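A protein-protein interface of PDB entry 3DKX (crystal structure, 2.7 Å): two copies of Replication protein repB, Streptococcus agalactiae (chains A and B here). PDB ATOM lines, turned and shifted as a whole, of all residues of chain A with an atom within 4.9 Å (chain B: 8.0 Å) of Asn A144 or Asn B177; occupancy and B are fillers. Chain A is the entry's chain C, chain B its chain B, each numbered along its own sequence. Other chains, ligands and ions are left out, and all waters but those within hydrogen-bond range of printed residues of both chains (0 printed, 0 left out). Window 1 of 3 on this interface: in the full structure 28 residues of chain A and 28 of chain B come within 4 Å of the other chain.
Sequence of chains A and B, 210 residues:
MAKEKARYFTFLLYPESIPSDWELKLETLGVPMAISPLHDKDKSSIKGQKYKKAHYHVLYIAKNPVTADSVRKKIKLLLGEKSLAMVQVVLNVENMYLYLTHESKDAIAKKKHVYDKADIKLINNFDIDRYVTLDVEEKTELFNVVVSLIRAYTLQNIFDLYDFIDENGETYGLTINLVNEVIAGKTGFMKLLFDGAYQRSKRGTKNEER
The side-chain amide nitrogen (ND2) of Asn B180 sits close to the side-chain amide nitrogen (ND2) of Asn A144 (2.5 Å).
Of the 15 printed residues of chain B, 3 touch a printed residue of chain A.
Hydrophobic or aromatic side chains of chain B within 4 Å of the printed part of chain A: Tyr B162.
Printed residues of chain A that touch a printed residue of chain B: Asn A144 and Val A147.
Hydrophobic or aromatic side chains of chain A that line the printed part of chain B: Val A147.
No position is printed for both chains.
Of the 3 pairs that touch across the chains among the printed residues, none has its exchanged pair printed and touching as well.
Asn A144 touches just these residues of chain B: Asn B177 and Asn B180.
Printed residues of chain B within 4 Å of Val A147: Tyr B162 (3.6 Å).
Ile B176 touches none of the printed residues of chain A.
Asn B177 touches just one residue of chain A: Asn A144 (3.4 Å).
Printed residues of chain A within 4 Å of Asn B180: Asn A144.
Ala B184 touches none of the printed residues of chain A.
The nearest printed residue of chain A that does not touch Asn B177 is Val A145 (6.3 Å).
O of Thr A140 sits close to OD1 of Asn A144 (3.4 Å).
OH of Tyr B162 is in hydrogen-bond range of OD1 of Asn B180 (2.6 Å).
Among the printed residues, pairs that only touch across the chains: Asn A144 with Asn B177 and Val A147 with Tyr B162.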
ATOM      1  N   THR A 140      33.167   3.595   0.477  1.00  0.00           N
ATOM      2  CA  THR A 140      32.443   3.556   1.738  1.00  0.00           C
ATOM      3  C   THR A 140      33.238   2.818   2.823  1.00  0.00           C
ATOM      4  O   THR A 140      33.347   3.287   3.953  1.00  0.00           O
ATOM      5  CB  THR A 140      31.090   2.887   1.575  1.00  0.00           C
ATOM      6  OG1 THR A 140      30.363   3.513   0.520  1.00  0.00           O
ATOM      7  CG2 THR A 140      30.279   2.956   2.890  1.00  0.00           C
ATOM      8  N   GLU A 141      33.775   1.646   2.478  1.00  0.00           N
ATOM      9  CA  GLU A 141      34.627   0.882   3.397  1.00  0.00           C
ATOM     10  C   GLU A 141      35.718   1.784   3.981  1.00  0.00           C
ATOM     11  O   GLU A 141      35.849   1.925   5.191  1.00  0.00           O
ATOM     12  CB  GLU A 141      35.282  -0.274   2.653  1.00  0.00           C
ATOM     13  CG  GLU A 141      34.905  -1.619   3.154  1.00  0.00           C
ATOM     14  CD  GLU A 141      35.538  -2.742   2.333  1.00  0.00           C
ATOM     15  OE1 GLU A 141      36.740  -2.898   2.236  1.00  0.00           O
ATOM     16  OE2 GLU A 141      34.852  -3.534   1.748  1.00  0.00           O
ATOM     17  N   LEU A 142      36.501   2.408   3.104  1.00  0.00           N
ATOM     18  CA  LEU A 142      37.665   3.144   3.553  1.00  0.00           C
ATOM     19  C   LEU A 142      37.211   4.365   4.332  1.00  0.00           C
ATOM     20  O   LEU A 142      37.851   4.777   5.320  1.00  0.00           O
ATOM     21  CB  LEU A 142      38.558   3.523   2.372  1.00  0.00           C
ATOM     22  CG  LEU A 142      39.398   2.359   1.825  1.00  0.00           C
ATOM     23  CD1 LEU A 142      40.041   2.670   0.505  1.00  0.00           C
ATOM     24  CD2 LEU A 142      40.435   1.960   2.844  1.00  0.00           C
ATOM     25  N   PHE A 143      36.085   4.938   3.929  1.00  0.00           N
ATOM     26  CA  PHE A 143      35.594   6.043   4.697  1.00  0.00           C
ATOM     27  C   PHE A 143      35.296   5.654   6.145  1.00  0.00           C
ATOM     28  O   PHE A 143      35.638   6.406   7.074  1.00  0.00           O
ATOM     29  CB  PHE A 143      34.378   6.713   4.082  1.00  0.00           C
ATOM     30  CG  PHE A 143      33.963   7.945   4.842  1.00  0.00           C
ATOM     31  CD1 PHE A 143      34.697   9.111   4.755  1.00  0.00           C
ATOM     32  CD2 PHE A 143      32.901   7.905   5.712  1.00  0.00           C
ATOM     33  CE1 PHE A 143      34.349  10.243   5.496  1.00  0.00           C
ATOM     34  CE2 PHE A 143      32.523   9.037   6.449  1.00  0.00           C
ATOM     35  CZ  PHE A 143      33.260  10.210   6.340  1.00  0.00           C
ATOM     36  N   ASN A 144      34.653   4.501   6.353  1.00  0.00           N
ATOM     37  CA  ASN A 144      34.392   4.026   7.706  1.00  0.00           C
ATOM     38  C   ASN A 144      35.696   3.757   8.487  1.00  0.00           C
ATOM     39  O   ASN A 144      35.781   4.014   9.699  1.00  0.00           O
ATOM     40  CB  ASN A 144      33.530   2.781   7.672  1.00  0.00           C
ATOM     41  CG  ASN A 144      32.096   3.056   7.229  1.00  0.00           C
ATOM     42  OD1 ASN A 144      31.456   2.209   6.595  1.00  0.00           O
ATOM     43  ND2 ASN A 144      31.579   4.240   7.572  1.00  0.00           N
ATOM     44  N   VAL A 145      36.713   3.228   7.810  1.00  0.00           N
ATOM     45  CA  VAL A 145      37.992   3.048   8.469  1.00  0.00           C
ATOM     46  C   VAL A 145      38.504   4.419   8.923  1.00  0.00           C
ATOM     47  O   VAL A 145      38.976   4.589  10.066  1.00  0.00           O
ATOM     48  CB  VAL A 145      39.030   2.418   7.546  1.00  0.00           C
ATOM     49  CG1 VAL A 145      40.393   2.520   8.172  1.00  0.00           C
ATOM     50  CG2 VAL A 145      38.662   0.988   7.249  1.00  0.00           C
ATOM     51  N   VAL A 146      38.421   5.401   8.034  1.00  0.00           N
ATOM     52  CA  VAL A 146      38.923   6.721   8.383  1.00  0.00           C
ATOM     53  C   VAL A 146      38.168   7.260   9.601  1.00  0.00           C
ATOM     54  O   VAL A 146      38.749   7.919  10.465  1.00  0.00           O
ATOM     55  CB  VAL A 146      38.760   7.712   7.213  1.00  0.00           C
ATOM     56  CG1 VAL A 146      38.931   9.144   7.702  1.00  0.00           C
ATOM     57  CG2 VAL A 146      39.726   7.368   6.072  1.00  0.00           C
ATOM     58  N   VAL A 147      36.871   6.989   9.676  1.00  0.00           N
ATOM     59  CA  VAL A 147      36.117   7.424  10.832  1.00  0.00           C
ATOM     60  C   VAL A 147      36.687   6.754  12.102  1.00  0.00           C
ATOM     61  O   VAL A 147      36.989   7.417  13.092  1.00  0.00           O
ATOM     62  CB  VAL A 147      34.620   7.074  10.680  1.00  0.00           C
ATOM     63  CG1 VAL A 147      33.848   7.321  11.995  1.00  0.00           C
ATOM     64  CG2 VAL A 147      33.997   7.819   9.502  1.00  0.00           C
ATOM     65  N   SER A 148      36.848   5.440  12.090  1.00  0.00           N
ATOM     66  CA  SER A 148      37.318   4.798  13.306  1.00  0.00           C
ATOM     67  C   SER A 148      38.688   5.316  13.731  1.00  0.00           C
ATOM     68  O   SER A 148      38.927   5.537  14.922  1.00  0.00           O
ATOM     69  CB  SER A 148      37.317   3.276  13.186  1.00  0.00           C
ATOM     70  OG  SER A 148      38.241   2.858  12.221  1.00  0.00           O
ATOM     71  N   ASP B 129      27.990  -7.386   3.330  1.00  0.00           N
ATOM     72  CA  ASP B 129      27.586  -6.217   4.081  1.00  0.00           C
ATOM     73  C   ASP B 129      27.633  -4.941   3.241  1.00  0.00           C
ATOM     74  O   ASP B 129      26.872  -4.013   3.495  1.00  0.00           O
ATOM     75  CB  ASP B 129      28.418  -6.055   5.355  1.00  0.00           C
ATOM     76  CG  ASP B 129      27.800  -6.779   6.569  1.00  0.00           C
ATOM     77  OD1 ASP B 129      26.550  -6.754   6.729  1.00  0.00           O
ATOM     78  OD2 ASP B 129      28.570  -7.355   7.381  1.00  0.00           O
ATOM     79  N   LEU B 134      20.406   0.514   2.662  1.00  0.00           N
ATOM     80  CA  LEU B 134      19.061   0.923   3.049  1.00  0.00           C
ATOM     81  C   LEU B 134      18.232   1.466   1.880  1.00  0.00           C
ATOM     82  O   LEU B 134      18.772   2.087   0.983  1.00  0.00           O
ATOM     83  CB  LEU B 134      19.161   1.961   4.155  1.00  0.00           C
ATOM     84  CG  LEU B 134      19.992   1.561   5.384  1.00  0.00           C
ATOM     85  CD1 LEU B 134      20.415   2.792   6.198  1.00  0.00           C
ATOM     86  CD2 LEU B 134      19.224   0.591   6.271  1.00  0.00           C
ATOM     87  N   TYR B 162      28.297   8.646  18.654  1.00  0.00           N
ATOM     88  CA  TYR B 162      28.929   7.386  18.367  1.00  0.00           C
ATOM     89  C   TYR B 162      28.992   6.535  19.627  1.00  0.00           C
ATOM     90  O   TYR B 162      28.629   5.355  19.604  1.00  0.00           O
ATOM     91  CB  TYR B 162      30.321   7.609  17.798  1.00  0.00           C
ATOM     92  CG  TYR B 162      30.332   7.890  16.306  1.00  0.00           C
ATOM     93  CD1 TYR B 162      29.425   7.262  15.448  1.00  0.00           C
ATOM     94  CD2 TYR B 162      31.268   8.750  15.750  1.00  0.00           C
ATOM     95  CE1 TYR B 162      29.457   7.508  14.082  1.00  0.00           C
ATOM     96  CE2 TYR B 162      31.300   8.990  14.393  1.00  0.00           C
ATOM     97  CZ  TYR B 162      30.397   8.375  13.564  1.00  0.00           C
ATOM     98  OH  TYR B 162      30.455   8.607  12.207  1.00  0.00           O
ATOM     99  N   ILE B 165      25.911   4.989  20.565  1.00  0.00           N
ATOM    100  CA  ILE B 165      25.522   3.875  19.706  1.00  0.00           C
ATOM    101  C   ILE B 165      26.264   2.623  20.113  1.00  0.00           C
ATOM    102  O   ILE B 165      25.723   1.517  20.060  1.00  0.00           O
ATOM    103  CB  ILE B 165      25.804   4.130  18.211  1.00  0.00           C
ATOM    104  CG1 ILE B 165      24.965   5.293  17.695  1.00  0.00           C
ATOM    105  CG2 ILE B 165      25.461   2.893  17.404  1.00  0.00           C
ATOM    106  CD1 ILE B 165      23.481   4.964  17.572  1.00  0.00           C
ATOM    107  N   LEU B 174      20.636   0.280  15.451  1.00  0.00           N
ATOM    108  CA  LEU B 174      21.698   1.089  14.891  1.00  0.00           C
ATOM    109  C   LEU B 174      23.098   0.516  15.113  1.00  0.00           C
ATOM    110  O   LEU B 174      23.351  -0.167  16.095  1.00  0.00           O
ATOM    111  CB  LEU B 174      21.626   2.494  15.481  1.00  0.00           C
ATOM    112  CG  LEU B 174      20.478   3.347  14.917  1.00  0.00           C
ATOM    113  CD1 LEU B 174      20.381   4.712  15.612  1.00  0.00           C
ATOM    114  CD2 LEU B 174      20.652   3.498  13.401  1.00  0.00           C
ATOM    115  N   THR B 175      24.007   0.818  14.188  1.00  0.00           N
ATOM    116  CA  THR B 175      25.423   0.517  14.341  1.00  0.00           C
ATOM    117  C   THR B 175      26.197   1.727  13.911  1.00  0.00           C
ATOM    118  O   THR B 175      25.644   2.622  13.285  1.00  0.00           O
ATOM    119  CB  THR B 175      25.894  -0.551  13.342  1.00  0.00           C
ATOM    120  OG1 THR B 175      24.940  -0.666  12.287  1.00  0.00           O
ATOM    121  CG2 THR B 175      26.023  -1.892  14.003  1.00  0.00           C
ATOM    122  N   ILE B 176      27.496   1.721  14.186  1.00  0.00           N
ATOM    123  CA  ILE B 176      28.374   2.763  13.689  1.00  0.00           C
ATOM    124  C   ILE B 176      28.258   2.919  12.157  1.00  0.00           C
ATOM    125  O   ILE B 176      27.841   3.956  11.662  1.00  0.00           O
ATOM    126  CB  ILE B 176      29.832   2.528  14.102  1.00  0.00           C
ATOM    127  CG1 ILE B 176      29.976   2.492  15.627  1.00  0.00           C
ATOM    128  CG2 ILE B 176      30.693   3.619  13.546  1.00  0.00           C
ATOM    129  CD1 ILE B 176      29.283   3.636  16.361  1.00  0.00           C
ATOM    130  N   ASN B 177      28.600   1.888  11.409  1.00  0.00           N
ATOM    131  CA  ASN B 177      28.481   1.969   9.961  1.00  0.00           C
ATOM    132  C   ASN B 177      27.081   2.343   9.468  1.00  0.00           C
ATOM    133  O   ASN B 177      26.923   2.980   8.420  1.00  0.00           O
ATOM    134  CB  ASN B 177      28.969   0.677   9.317  1.00  0.00           C
ATOM    135  CG  ASN B 177      30.468   0.491   9.483  1.00  0.00           C
ATOM    136  OD1 ASN B 177      31.167   1.369  10.014  1.00  0.00           O
ATOM    137  ND2 ASN B 177      30.972  -0.646   9.038  1.00  0.00           N
ATOM    138  N   LEU B 178      26.054   1.967  10.212  1.00  0.00           N
ATOM    139  CA  LEU B 178      24.695   2.248   9.771  1.00  0.00           C
ATOM    140  C   LEU B 178      24.380   3.711  10.003  1.00  0.00           C
ATOM    141  O   LEU B 178      23.752   4.374   9.162  1.00  0.00           O
ATOM    142  CB  LEU B 178      23.696   1.378  10.517  1.00  0.00           C
ATOM    143  CG  LEU B 178      22.506   0.848   9.721  1.00  0.00           C
ATOM    144  CD1 LEU B 178      22.908   0.416   8.316  1.00  0.00           C
ATOM    145  CD2 LEU B 178      21.882  -0.310  10.491  1.00  0.00           C
ATOM    146  N   VAL B 179      24.803   4.229  11.144  1.00  0.00           N
ATOM    147  CA  VAL B 179      24.689   5.666  11.355  1.00  0.00           C
ATOM    148  C   VAL B 179      25.385   6.442  10.223  1.00  0.00           C
ATOM    149  O   VAL B 179      24.793   7.365   9.644  1.00  0.00           O
ATOM    150  CB  VAL B 179      25.276   6.093  12.695  1.00  0.00           C
ATOM    151  CG1 VAL B 179      25.436   7.588  12.742  1.00  0.00           C
ATOM    152  CG2 VAL B 179      24.365   5.645  13.834  1.00  0.00           C
ATOM    153  N   ASN B 180      26.624   6.070   9.898  1.00  0.00           N
ATOM    154  CA  ASN B 180      27.324   6.684   8.774  1.00  0.00           C
ATOM    155  C   ASN B 180      26.524   6.656   7.480  1.00  0.00           C
ATOM    156  O   ASN B 180      26.545   7.609   6.724  1.00  0.00           O
ATOM    157  CB  ASN B 180      28.672   6.043   8.514  1.00  0.00           C
ATOM    158  CG  ASN B 180      29.614   6.201   9.650  1.00  0.00           C
ATOM    159  OD1 ASN B 180      29.381   6.954  10.588  1.00  0.00           O
ATOM    160  ND2 ASN B 180      30.696   5.474   9.588  1.00  0.00           N
ATOM    161  N   GLU B 181      25.842   5.558   7.199  1.00  0.00           N
ATOM    162  CA  GLU B 181      25.105   5.465   5.939  1.00  0.00           C
ATOM    163  C   GLU B 181      23.864   6.322   6.040  1.00  0.00           C
ATOM    164  O   GLU B 181      23.356   6.849   5.053  1.00  0.00           O
ATOM    165  CB  GLU B 181      24.690   4.012   5.649  1.00  0.00           C
ATOM    166  CG  GLU B 181      23.944   3.842   4.336  1.00  0.00           C
ATOM    167  CD  GLU B 181      23.446   2.411   4.116  1.00  0.00           C
ATOM    168  OE1 GLU B 181      23.724   1.547   4.987  1.00  0.00           O
ATOM    169  OE2 GLU B 181      22.772   2.154   3.075  1.00  0.00           O
ATOM    170  N   VAL B 182      23.362   6.451   7.258  1.00  0.00           N
ATOM    171  CA  VAL B 182      22.100   7.140   7.467  1.00  0.00           C
ATOM    172  C   VAL B 182      22.341   8.636   7.379  1.00  0.00           C
ATOM    173  O   VAL B 182      21.608   9.348   6.706  1.00  0.00           O
ATOM    174  CB  VAL B 182      21.453   6.717   8.826  1.00  0.00           C
ATOM    175  CG1 VAL B 182      20.415   7.712   9.290  1.00  0.00           C
ATOM    176  CG2 VAL B 182      20.858   5.315   8.697  1.00  0.00           C
ATOM    177  N   ILE B 183      23.371   9.132   8.042  1.00  0.00           N
ATOM    178  CA  ILE B 183      23.559  10.564   8.019  1.00  0.00           C
ATOM    179  C   ILE B 183      24.306  11.094   6.815  1.00  0.00           C
ATOM    180  O   ILE B 183      24.443  12.306   6.713  1.00  0.00           O
ATOM    181  CB  ILE B 183      24.263  11.128   9.279  1.00  0.00           C
ATOM    182  CG1 ILE B 183      25.729  10.766   9.321  1.00  0.00           C
ATOM    183  CG2 ILE B 183      23.613  10.643  10.577  1.00  0.00           C
ATOM    184  CD1 ILE B 183      26.272  10.960  10.744  1.00  0.00           C
ATOM    185  N   ALA B 184      24.769  10.229   5.904  1.00  0.00           N
ATOM    186  CA  ALA B 184      25.390  10.707   4.675  1.00  0.00           C
ATOM    187  C   ALA B 184      24.428  11.658   3.989  1.00  0.00           C
ATOM    188  O   ALA B 184      23.209  11.431   3.999  1.00  0.00           O
ATOM    189  CB  ALA B 184      25.718   9.551   3.745  1.00  0.00           C
